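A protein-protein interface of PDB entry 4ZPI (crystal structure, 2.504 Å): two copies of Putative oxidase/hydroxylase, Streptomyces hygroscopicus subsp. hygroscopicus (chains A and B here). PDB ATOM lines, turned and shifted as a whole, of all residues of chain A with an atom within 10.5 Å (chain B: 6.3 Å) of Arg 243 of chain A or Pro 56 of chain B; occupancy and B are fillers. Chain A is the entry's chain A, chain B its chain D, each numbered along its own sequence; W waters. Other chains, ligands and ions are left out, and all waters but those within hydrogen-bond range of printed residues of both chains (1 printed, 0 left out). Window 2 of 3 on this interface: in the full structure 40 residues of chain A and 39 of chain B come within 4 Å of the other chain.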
ATOM      1  N   THR A 230      -9.823 -11.782 -18.064  1.00  0.00           N
ATOM      2  CA  THR A 230     -10.561 -11.581 -19.317  1.00  0.00           C
ATOM      3  C   THR A 230     -11.802 -10.782 -19.029  1.00  0.00           C
ATOM      4  O   THR A 230     -12.290 -10.806 -17.898  1.00  0.00           O
ATOM      5  CB  THR A 230     -11.014 -12.882 -19.987  1.00  0.00           C
ATOM      6  OG1 THR A 230     -11.717 -13.690 -19.028  1.00  0.00           O
ATOM      7  CG2 THR A 230      -9.844 -13.643 -20.567  1.00  0.00           C
ATOM      8  N   ARG A 233     -17.629 -12.944 -18.919  1.00  0.00           N
ATOM      9  CA  ARG A 233     -18.380 -13.808 -19.805  1.00  0.00           C
ATOM     10  C   ARG A 233     -18.684 -15.047 -18.993  1.00  0.00           C
ATOM     11  O   ARG A 233     -17.821 -15.525 -18.247  1.00  0.00           O
ATOM     12  CB  ARG A 233     -17.581 -14.155 -21.061  1.00  0.00           C
ATOM     13  CG  ARG A 233     -18.364 -14.053 -22.356  1.00  0.00           C
ATOM     14  CD  ARG A 233     -17.642 -14.749 -23.513  1.00  0.00           C
ATOM     15  NE  ARG A 233     -17.492 -16.185 -23.273  1.00  0.00           N
ATOM     16  CZ  ARG A 233     -17.408 -17.108 -24.230  1.00  0.00           C
ATOM     17  NH1 ARG A 233     -17.463 -16.748 -25.511  1.00  0.00           N
ATOM     18  NH2 ARG A 233     -17.275 -18.392 -23.902  1.00  0.00           N
ATOM     19  N   LEU A 235     -19.247 -18.976 -18.443  1.00  0.00           N
ATOM     20  CA  LEU A 235     -18.746 -20.189 -19.036  1.00  0.00           C
ATOM     21  C   LEU A 235     -19.295 -21.342 -18.217  1.00  0.00           C
ATOM     22  O   LEU A 235     -19.138 -21.354 -16.996  1.00  0.00           O
ATOM     23  CB  LEU A 235     -17.220 -20.174 -19.050  1.00  0.00           C
ATOM     24  CG  LEU A 235     -16.486 -21.440 -19.463  1.00  0.00           C
ATOM     25  CD1 LEU A 235     -16.679 -21.709 -20.945  1.00  0.00           C
ATOM     26  CD2 LEU A 235     -15.030 -21.286 -19.116  1.00  0.00           C
ATOM     27  N   ALA A 237     -18.425 -24.480 -18.186  1.00  0.00           N
ATOM     28  CA  ALA A 237     -17.357 -25.311 -17.665  1.00  0.00           C
ATOM     29  C   ALA A 237     -16.104 -25.208 -18.503  1.00  0.00           C
ATOM     30  O   ALA A 237     -16.100 -24.632 -19.587  1.00  0.00           O
ATOM     31  CB  ALA A 237     -17.798 -26.744 -17.594  1.00  0.00           C
ATOM     32  N   GLU A 238     -15.030 -25.773 -17.974  1.00  0.00           N
ATOM     33  CA  GLU A 238     -13.800 -25.931 -18.722  1.00  0.00           C
ATOM     34  C   GLU A 238     -14.079 -26.655 -20.040  1.00  0.00           C
ATOM     35  O   GLU A 238     -14.804 -27.645 -20.069  1.00  0.00           O
ATOM     36  CB  GLU A 238     -12.780 -26.699 -17.876  1.00  0.00           C
ATOM     37  CG  GLU A 238     -11.711 -27.399 -18.677  1.00  0.00           C
ATOM     38  CD  GLU A 238     -10.967 -28.425 -17.852  1.00  0.00           C
ATOM     39  OE1 GLU A 238     -10.443 -28.049 -16.778  1.00  0.00           O
ATOM     40  OE2 GLU A 238     -10.923 -29.607 -18.269  1.00  0.00           O
ATOM     41  N   THR A 239     -13.520 -26.151 -21.132  1.00  0.00           N
ATOM     42  CA  THR A 239     -13.681 -26.806 -22.425  1.00  0.00           C
ATOM     43  C   THR A 239     -12.623 -27.890 -22.629  1.00  0.00           C
ATOM     44  O   THR A 239     -11.580 -27.900 -21.956  1.00  0.00           O
ATOM     45  CB  THR A 239     -13.611 -25.800 -23.560  1.00  0.00           C
ATOM     46  OG1 THR A 239     -12.258 -25.381 -23.732  1.00  0.00           O
ATOM     47  CG2 THR A 239     -14.474 -24.591 -23.240  1.00  0.00           C
ATOM     48  N   ALA A 240     -12.887 -28.809 -23.548  1.00  0.00           N
ATOM     49  CA  ALA A 240     -12.061 -30.012 -23.668  1.00  0.00           C
ATOM     50  C   ALA A 240     -10.665 -29.705 -24.206  1.00  0.00           C
ATOM     51  O   ALA A 240      -9.698 -30.408 -23.874  1.00  0.00           O
ATOM     52  CB  ALA A 240     -12.750 -31.049 -24.552  1.00  0.00           C
ATOM     53  N   ASP A 241     -10.556 -28.653 -25.014  1.00  0.00           N
ATOM     54  CA  ASP A 241      -9.268 -28.270 -25.603  1.00  0.00           C
ATOM     55  C   ASP A 241      -8.534 -27.241 -24.772  1.00  0.00           C
ATOM     56  O   ASP A 241      -7.535 -26.696 -25.219  1.00  0.00           O
ATOM     57  CB  ASP A 241      -9.464 -27.715 -27.011  1.00  0.00           C
ATOM     58  CG  ASP A 241     -10.388 -26.509 -27.039  1.00  0.00           C
ATOM     59  OD1 ASP A 241     -11.112 -26.287 -26.046  1.00  0.00           O
ATOM     60  OD2 ASP A 241     -10.406 -25.790 -28.060  1.00  0.00           O
ATOM     61  N   LEU A 242      -9.063 -26.969 -23.582  1.00  0.00           N
ATOM     62  CA  LEU A 242      -8.524 -25.976 -22.653  1.00  0.00           C
ATOM     63  C   LEU A 242      -8.430 -24.561 -23.230  1.00  0.00           C
ATOM     64  O   LEU A 242      -7.600 -23.765 -22.795  1.00  0.00           O
ATOM     65  CB  LEU A 242      -7.142 -26.417 -22.155  1.00  0.00           C
ATOM     66  CG  LEU A 242      -7.162 -27.652 -21.270  1.00  0.00           C
ATOM     67  CD1 LEU A 242      -5.815 -27.829 -20.598  1.00  0.00           C
ATOM     68  CD2 LEU A 242      -8.273 -27.523 -20.243  1.00  0.00           C
ATOM     69  N   ARG A 243      -9.287 -24.232 -24.188  1.00  0.00           N
ATOM     70  CA  ARG A 243      -9.148 -22.954 -24.880  1.00  0.00           C
ATOM     71  C   ARG A 243     -10.248 -21.951 -24.544  1.00  0.00           C
ATOM     72  O   ARG A 243     -10.134 -20.773 -24.868  1.00  0.00           O
ATOM     73  CB  ARG A 243      -9.099 -23.182 -26.384  1.00  0.00           C
ATOM     74  CG  ARG A 243      -7.766 -22.836 -27.003  1.00  0.00           C
ATOM     75  CD  ARG A 243      -6.752 -23.889 -26.720  1.00  0.00           C
ATOM     76  NE  ARG A 243      -5.515 -23.653 -27.458  1.00  0.00           N
ATOM     77  CZ  ARG A 243      -4.587 -24.582 -27.685  1.00  0.00           C
ATOM     78  NH1 ARG A 243      -4.749 -25.829 -27.237  1.00  0.00           N
ATOM     79  NH2 ARG A 243      -3.497 -24.264 -28.370  1.00  0.00           N
ATOM     80  N   GLY A 244     -11.295 -22.420 -23.873  1.00  0.00           N
ATOM     81  CA  GLY A 244     -12.409 -21.574 -23.480  1.00  0.00           C
ATOM     82  C   GLY A 244     -12.136 -20.625 -22.321  1.00  0.00           C
ATOM     83  O   GLY A 244     -11.662 -21.036 -21.252  1.00  0.00           O
ATOM     84  N   ALA A 245     -12.460 -19.351 -22.537  1.00  0.00           N
ATOM     85  CA  ALA A 245     -12.232 -18.296 -21.558  1.00  0.00           C
ATOM     86  C   ALA A 245     -13.535 -17.867 -20.887  1.00  0.00           C
ATOM     87  O   ALA A 245     -14.593 -17.921 -21.506  1.00  0.00           O
ATOM     88  CB  ALA A 245     -11.579 -17.111 -22.224  1.00  0.00           C
ATOM     89  N   GLY A 246     -13.455 -17.436 -19.628  1.00  0.00           N
ATOM     90  CA  GLY A 246     -14.629 -16.963 -18.917  1.00  0.00           C
ATOM     91  C   GLY A 246     -14.742 -17.423 -17.476  1.00  0.00           C
ATOM     92  O   GLY A 246     -13.849 -18.089 -16.945  1.00  0.00           O
ATOM     93  N   PRO B  53       7.661 -19.207 -30.194  1.00  0.00           N
ATOM     94  CA  PRO B  53       6.360 -18.750 -29.683  1.00  0.00           C
ATOM     95  C   PRO B  53       5.174 -19.544 -30.218  1.00  0.00           C
ATOM     96  O   PRO B  53       5.164 -19.934 -31.383  1.00  0.00           O
ATOM     97  CB  PRO B  53       6.298 -17.304 -30.162  1.00  0.00           C
ATOM     98  CG  PRO B  53       7.118 -17.301 -31.407  1.00  0.00           C
ATOM     99  CD  PRO B  53       8.257 -18.237 -31.125  1.00  0.00           C
ATOM    100  N   ASP B  54       4.194 -19.772 -29.351  1.00  0.00           N
ATOM    101  CA  ASP B  54       2.937 -20.460 -29.683  1.00  0.00           C
ATOM    102  C   ASP B  54       3.119 -21.782 -30.441  1.00  0.00           C
ATOM    103  O   ASP B  54       2.714 -21.920 -31.595  1.00  0.00           O
ATOM    104  CB  ASP B  54       2.017 -19.529 -30.482  1.00  0.00           C
ATOM    105  CG  ASP B  54       0.557 -19.948 -30.397  1.00  0.00           C
ATOM    106  OD1 ASP B  54       0.274 -21.020 -29.804  1.00  0.00           O
ATOM    107  OD2 ASP B  54      -0.308 -19.216 -30.933  1.00  0.00           O
ATOM    108  N   LEU B  55       3.717 -22.757 -29.769  1.00  0.00           N
ATOM    109  CA  LEU B  55       3.939 -24.072 -30.358  1.00  0.00           C
ATOM    110  C   LEU B  55       2.652 -24.826 -30.722  1.00  0.00           C
ATOM    111  O   LEU B  55       2.583 -25.408 -31.805  1.00  0.00           O
ATOM    112  CB  LEU B  55       4.787 -24.940 -29.421  1.00  0.00           C
ATOM    113  CG  LEU B  55       6.281 -24.686 -29.434  1.00  0.00           C
ATOM    114  CD1 LEU B  55       6.975 -25.707 -28.538  1.00  0.00           C
ATOM    115  CD2 LEU B  55       6.804 -24.750 -30.857  1.00  0.00           C
ATOM    116  N   PRO B  56       1.643 -24.852 -29.824  1.00  0.00           N
ATOM    117  CA  PRO B  56       0.438 -25.608 -30.204  1.00  0.00           C
ATOM    118  C   PRO B  56      -0.171 -25.157 -31.535  1.00  0.00           C
ATOM    119  O   PRO B  56      -0.479 -25.990 -32.390  1.00  0.00           O
ATOM    120  CB  PRO B  56      -0.527 -25.331 -29.049  1.00  0.00           C
ATOM    121  CG  PRO B  56       0.342 -25.037 -27.893  1.00  0.00           C
ATOM    122  CD  PRO B  56       1.571 -24.372 -28.427  1.00  0.00           C
ATOM    123  N   ALA B  57      -0.313 -23.851 -31.717  1.00  0.00           N
ATOM    124  CA  ALA B  57      -0.876 -23.329 -32.955  1.00  0.00           C
ATOM    125  C   ALA B  57       0.019 -23.638 -34.161  1.00  0.00           C
ATOM    126  O   ALA B  57      -0.449 -23.634 -35.295  1.00  0.00           O
ATOM    127  CB  ALA B  57      -1.105 -21.834 -32.837  1.00  0.00           C
ATOM    128  N   ALA B  58       1.295 -23.928 -33.913  1.00  0.00           N
ATOM    129  CA  ALA B  58       2.264 -24.084 -34.998  1.00  0.00           C
ATOM    130  C   ALA B  58       2.551 -25.543 -35.343  1.00  0.00           C
ATOM    131  O   ALA B  58       3.231 -25.825 -36.330  1.00  0.00           O
ATOM    132  CB  ALA B  58       3.574 -23.368 -34.643  1.00  0.00           C
ATOM    133  N   SER B  59       2.041 -26.470 -34.538  1.00  0.00           N
ATOM    134  CA  SER B  59       2.415 -27.870 -34.700  1.00  0.00           C
ATOM    135  C   SER B  59       1.486 -28.830 -33.962  1.00  0.00           C
ATOM    136  O   SER B  59       1.305 -28.715 -32.747  1.00  0.00           O
ATOM    137  CB  SER B  59       3.856 -28.078 -34.218  1.00  0.00           C
ATOM    138  OG  SER B  59       4.123 -29.449 -33.981  1.00  0.00           O
ATOM    139  N   PRO B  60       0.909 -29.799 -34.696  1.00  0.00           N
ATOM    140  CA  PRO B  60      -0.007 -30.799 -34.121  1.00  0.00           C
ATOM    141  C   PRO B  60       0.610 -31.643 -33.006  1.00  0.00           C
ATOM    142  O   PRO B  60      -0.102 -32.078 -32.103  1.00  0.00           O
ATOM    143  CB  PRO B  60      -0.370 -31.684 -35.328  1.00  0.00           C
ATOM    144  CG  PRO B  60       0.673 -31.381 -36.370  1.00  0.00           C
ATOM    145  CD  PRO B  60       1.036 -29.947 -36.157  1.00  0.00           C
ATOM    146  N   PHE B  62       2.860 -30.672 -30.735  1.00  0.00           N
ATOM    147  CA  PHE B  62       2.856 -29.877 -29.515  1.00  0.00           C
ATOM    148  C   PHE B  62       1.450 -29.449 -29.078  1.00  0.00           C
ATOM    149  O   PHE B  62       1.239 -29.173 -27.895  1.00  0.00           O
ATOM    150  CB  PHE B  62       3.767 -28.661 -29.676  1.00  0.00           C
ATOM    151  CG  PHE B  62       5.218 -29.022 -29.787  1.00  0.00           C
ATOM    152  CD1 PHE B  62       5.855 -29.685 -28.753  1.00  0.00           C
ATOM    153  CD2 PHE B  62       5.942 -28.719 -30.921  1.00  0.00           C
ATOM    154  CE1 PHE B  62       7.176 -30.034 -28.853  1.00  0.00           C
ATOM    155  CE2 PHE B  62       7.267 -29.068 -31.023  1.00  0.00           C
ATOM    156  CZ  PHE B  62       7.885 -29.723 -29.987  1.00  0.00           C
ATOM    157  N   ALA B  63       0.493 -29.411 -30.007  1.00  0.00           N
ATOM    158  CA  ALA B  63      -0.916 -29.229 -29.639  1.00  0.00           C
ATOM    159  C   ALA B  63      -1.382 -30.405 -28.799  1.00  0.00           C
ATOM    160  O   ALA B  63      -2.083 -30.241 -27.800  1.00  0.00           O
ATOM    161  CB  ALA B  63      -1.784 -29.090 -30.862  1.00  0.00           C
ATOM    162  N   ARG B  64      -0.973 -31.600 -29.207  1.00  0.00           N
ATOM    163  CA  ARG B  64      -1.234 -32.799 -28.422  1.00  0.00           C
ATOM    164  C   ARG B  64      -0.496 -32.795 -27.083  1.00  0.00           C
ATOM    165  O   ARG B  64      -1.064 -33.180 -26.062  1.00  0.00           O
ATOM    166  CB  ARG B  64      -0.857 -34.056 -29.214  1.00  0.00           C
ATOM    167  CG  ARG B  64      -1.933 -34.509 -30.199  1.00  0.00           C
ATOM    168  CD  ARG B  64      -1.646 -35.913 -30.743  1.00  0.00           C
ATOM    169  NE  ARG B  64      -0.438 -35.940 -31.567  1.00  0.00           N
ATOM    170  CZ  ARG B  64      -0.374 -35.491 -32.818  1.00  0.00           C
ATOM    171  NH1 ARG B  64      -1.457 -34.979 -33.396  1.00  0.00           N
ATOM    172  NH2 ARG B  64       0.770 -35.554 -33.491  1.00  0.00           N
ATOM    173  N   ALA B  66       0.442 -30.344 -25.312  1.00  0.00           N
ATOM    174  CA  ALA B  66      -0.113 -29.337 -24.428  1.00  0.00           C
ATOM    175  C   ALA B  66      -1.305 -29.869 -23.655  1.00  0.00           C
ATOM    176  O   ALA B  66      -1.628 -29.369 -22.584  1.00  0.00           O
ATOM    177  CB  ALA B  66      -0.503 -28.103 -25.220  1.00  0.00           C
ATOM    178  N   LEU B  67      -1.957 -30.894 -24.201  1.00  0.00           N
ATOM    179  CA  LEU B  67      -3.157 -31.457 -23.585  1.00  0.00           C
ATOM    180  C   LEU B  67      -2.910 -32.889 -23.122  1.00  0.00           C
ATOM    181  O   LEU B  67      -3.827 -33.563 -22.655  1.00  0.00           O
ATOM    182  CB  LEU B  67      -4.342 -31.396 -24.553  1.00  0.00           C
ATOM    183  CG  LEU B  67      -4.679 -29.983 -25.069  1.00  0.00           C
ATOM    184  CD1 LEU B  67      -5.945 -29.968 -25.880  1.00  0.00           C
ATOM    185  CD2 LEU B  67      -4.781 -28.982 -23.925  1.00  0.00           C
ATOM    186  N   LEU B  83      -9.627 -25.082 -15.909  1.00  0.00           N
ATOM    187  CA  LEU B  83      -8.315 -24.837 -16.488  1.00  0.00           C
ATOM    188  C   LEU B  83      -8.338 -24.232 -17.907  1.00  0.00           C
ATOM    189  O   LEU B  83      -9.240 -24.507 -18.710  1.00  0.00           O
ATOM    190  CB  LEU B  83      -7.557 -26.156 -16.489  1.00  0.00           C
ATOM    191  CG  LEU B  83      -6.045 -26.196 -16.539  1.00  0.00           C
ATOM    192  CD1 LEU B  83      -5.467 -25.494 -15.320  1.00  0.00           C
ATOM    193  CD2 LEU B  83      -5.661 -27.663 -16.575  1.00  0.00           C
ATOM    194  N   ARG B  84      -7.345 -23.391 -18.199  1.00  0.00           N
ATOM    195  CA  ARG B  84      -7.163 -22.812 -19.529  1.00  0.00           C
ATOM    196  C   ARG B  84      -5.677 -22.818 -19.881  1.00  0.00           C
ATOM    197  O   ARG B  84      -4.827 -22.578 -19.015  1.00  0.00           O
ATOM    198  CB  ARG B  84      -7.724 -21.384 -19.599  1.00  0.00           C
ATOM    199  CG  ARG B  84      -7.642 -20.778 -20.997  1.00  0.00           C
ATOM    200  CD  ARG B  84      -8.050 -19.303 -21.056  1.00  0.00           C
ATOM    201  NE  ARG B  84      -8.064 -18.819 -22.442  1.00  0.00           N
ATOM    202  CZ  ARG B  84      -8.225 -17.547 -22.820  1.00  0.00           C
ATOM    203  NH1 ARG B  84      -8.391 -16.583 -21.924  1.00  0.00           N
ATOM    204  NH2 ARG B  84      -8.220 -17.235 -24.108  1.00  0.00           N
ATOM    205  N   LEU B  85      -5.359 -23.100 -21.142  1.00  0.00           N
ATOM    206  CA  LEU B  85      -3.975 -23.078 -21.604  1.00  0.00           C
ATOM    207  C   LEU B  85      -3.586 -21.658 -21.976  1.00  0.00           C
ATOM    208  O   LEU B  85      -4.155 -21.106 -22.900  1.00  0.00           O
ATOM    209  CB  LEU B  85      -3.780 -24.008 -22.804  1.00  0.00           C
ATOM    210  CG  LEU B  85      -2.412 -23.975 -23.494  1.00  0.00           C
ATOM    211  CD1 LEU B  85      -1.358 -24.773 -22.724  1.00  0.00           C
ATOM    212  CD2 LEU B  85      -2.511 -24.460 -24.927  1.00  0.00           C
ATOM    213  N   GLU B  87      -0.206 -20.299 -22.448  1.00  0.00           N
ATOM    214  CA  GLU B  87       0.952 -20.125 -23.312  1.00  0.00           C
ATOM    215  C   GLU B  87       1.657 -21.442 -23.558  1.00  0.00           C
ATOM    216  O   GLU B  87       1.494 -22.410 -22.807  1.00  0.00           O
ATOM    217  CB  GLU B  87       1.940 -19.118 -22.729  1.00  0.00           C
ATOM    218  CG  GLU B  87       2.607 -19.532 -21.441  1.00  0.00           C
ATOM    219  CD  GLU B  87       3.756 -18.595 -21.040  1.00  0.00           C
ATOM    220  OE1 GLU B  87       4.356 -17.957 -21.941  1.00  0.00           O
ATOM    221  OE2 GLU B  87       4.056 -18.491 -19.827  1.00  0.00           O
ATOM    222  N   GLY B  88       2.447 -21.467 -24.625  1.00  0.00           N
ATOM    223  CA  GLY B  88       3.162 -22.658 -25.034  1.00  0.00           C
ATOM    224  C   GLY B  88       4.281 -22.294 -25.986  1.00  0.00           C
ATOM    225  O   GLY B  88       4.045 -21.967 -27.147  1.00  0.00           O
ATOM    226  N   TYR B  89       5.511 -22.357 -25.497  1.00  0.00           N
ATOM    227  CA  TYR B  89       6.644 -21.944 -26.299  1.00  0.00           C
ATOM    228  C   TYR B  89       7.769 -22.950 -26.233  1.00  0.00           C
ATOM    229  O   TYR B  89       7.776 -23.847 -25.384  1.00  0.00           O
ATOM    230  CB  TYR B  89       7.144 -20.577 -25.848  1.00  0.00           C
ATOM    231  CG  TYR B  89       7.596 -20.540 -24.408  1.00  0.00           C
ATOM    232  CD1 TYR B  89       6.682 -20.353 -23.382  1.00  0.00           C
ATOM    233  CD2 TYR B  89       8.942 -20.677 -24.073  1.00  0.00           C
ATOM    234  CE1 TYR B  89       7.083 -20.310 -22.071  1.00  0.00           C
ATOM    235  CE2 TYR B  89       9.357 -20.630 -22.762  1.00  0.00           C
ATOM    236  CZ  TYR B  89       8.421 -20.448 -21.763  1.00  0.00           C
ATOM    237  OH  TYR B  89       8.812 -20.410 -20.444  1.00  0.00           O
ATOM    238  N   PHE B 222       4.745 -25.063 -21.179  1.00  0.00           N
ATOM    239  CA  PHE B 222       3.320 -24.820 -21.272  1.00  0.00           C
ATOM    240  C   PHE B 222       2.854 -24.221 -19.951  1.00  0.00           C
ATOM    241  O   PHE B 222       3.191 -24.730 -18.882  1.00  0.00           O
ATOM    242  CB  PHE B 222       2.590 -26.118 -21.629  1.00  0.00           C
ATOM    243  CG  PHE B 222       3.167 -26.798 -22.839  1.00  0.00           C
ATOM    244  CD1 PHE B 222       2.700 -26.496 -24.109  1.00  0.00           C
ATOM    245  CD2 PHE B 222       4.227 -27.697 -22.711  1.00  0.00           C
ATOM    246  CE1 PHE B 222       3.251 -27.094 -25.222  1.00  0.00           C
ATOM    247  CE2 PHE B 222       4.794 -28.302 -23.825  1.00  0.00           C
ATOM    248  CZ  PHE B 222       4.302 -28.004 -25.082  1.00  0.00           C
ATOM    249  N   GLU B 231      -4.818 -15.033 -22.107  1.00  0.00           N
ATOM    250  CA  GLU B 231      -3.603 -15.693 -22.589  1.00  0.00           C
ATOM    251  C   GLU B 231      -2.404 -14.787 -22.376  1.00  0.00           C
ATOM    252  O   GLU B 231      -2.535 -13.561 -22.430  1.00  0.00           O
ATOM    253  CB  GLU B 231      -3.710 -16.061 -24.065  1.00  0.00           C
ATOM    254  CG  GLU B 231      -4.598 -17.247 -24.337  1.00  0.00           C
ATOM    255  CD  GLU B 231      -4.859 -17.432 -25.823  1.00  0.00           C
ATOM    256  OE1 GLU B 231      -5.541 -18.427 -26.172  1.00  0.00           O
ATOM    257  OE2 GLU B 231      -4.394 -16.580 -26.632  1.00  0.00           O
HETATM  258  O   HOH W   1     -11.186 -24.188 -21.243  1.00  0.00           O
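Among the printed residues, pairs that only touch across the chains: Arg 243 of chain A with Pro 56 of chain B (3.2 Å), Ala 245 of chain A with Arg 84 of chain B (3.2 Å), Leu 242 of chain A with Arg 84 of chain B (3.4 Å), Arg 243 of chain A with Leu 85 of chain B (3.5 Å), Leu 242 of chain A with Leu 83 of chain B (3.5 Å), Thr 230 of chain A with Arg 84 of chain B (3.5 Å), Leu 242 of chain A with Leu 67 of chain B (3.7 Å), Asp 241 of chain A with Leu 67 of chain B (3.7 Å) and Arg 243 of chain A with Arg 84 of chain B (3.7 Å).
OG1 of Thr 239 of chain A lies within hydrogen-bond range of N of Arg 243 of chain A. The side-chain hydroxyl (OG1) of Thr 239 of chain A sits at hydrogen-bond distance from the side-chain carboxylate (OD1) of Asp 241 of chain A. OE1 of Glu 231 of chain B lies within salt-bridge range of NH2 of Arg 84 of chain B, 3.6 Å away. OD1 of Asp 241 of chain A sits close to N of Arg 243 of chain A (3.3 Å).
The backbone NH (N) of Leu 85 of chain B is in hydrogen-bond range of the backbone carbonyl oxygen (O) of Leu 242 of chain A (2.9 Å). OE1 of Glu 238 of chain A is in hydrogen-bond range of N of Leu 83 of chain B (3.2 Å).
Arg 243 of chain A touches three residues of chain B. Pro 56 of chain B touches one residue of chain A. No residue of chain A comes within 4 Å of Asp 54 of chain B. No residue of chain A comes within 4 Å of Leu 55 of chain B. No residue of chain A comes within 4 Å of Ala 58 of chain B. No residue of chain A comes within 4 Å of Ser 59 of chain B. No residue of chain A comes within 4 Å of Ala 63 of chain B. Of chain A, only Leu 242 (2.9 Å) and Arg 243 (3.5 Å) come within 4 Å of Leu 85 of chain B. No residue of chain A comes within 4 Å of Gly 88 of chain B. Of the printed residues of chain B, Asp 241 of chain A touches Leu 67. Of the printed residues of chain B, Leu 242 of chain A touches Leu 67 (3.7 Å), Leu 83 (3.5 Å), Arg 84 (3.4 Å) and Leu 85 (2.9 Å). Of the printed residues of chain B, Glu 238 of chain A touches Leu 83 (3.2 Å). The nearest residue of chain A that does not touch Pro 56 of chain B is Asp 241 of chain A (8.1 Å). The nearest printed residue of chain A that does not touch Arg 84 of chain B is Gly 244 of chain A (4.01 Å).
Printed residues of chain B that touch a printed residue of chain A: Pro 56, Leu 67, Leu 83, Arg 84 and Leu 85. Hydrophobic or aromatic side chains of chain B that line the printed part of chain A: Pro 56, Leu 67, Leu 83 and Leu 85. Along chain A the printed residues that touch a printed residue of chain B span positions 230 to 245. Among the printed residues, 11 pairs touch across the chains. Among the printed residues, no Asp or Glu carboxylate lies within 4 Å of a Lys or Arg side-chain nitrogen of the other chain.
No position is printed for both chains.
Water W1 lies within hydrogen-bond range of OG1 of Thr 239 of chain A (3.0 Å), N of Gly 244 of chain A (3.2 Å) and O of Leu 83 of chain B (3.2 Å).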
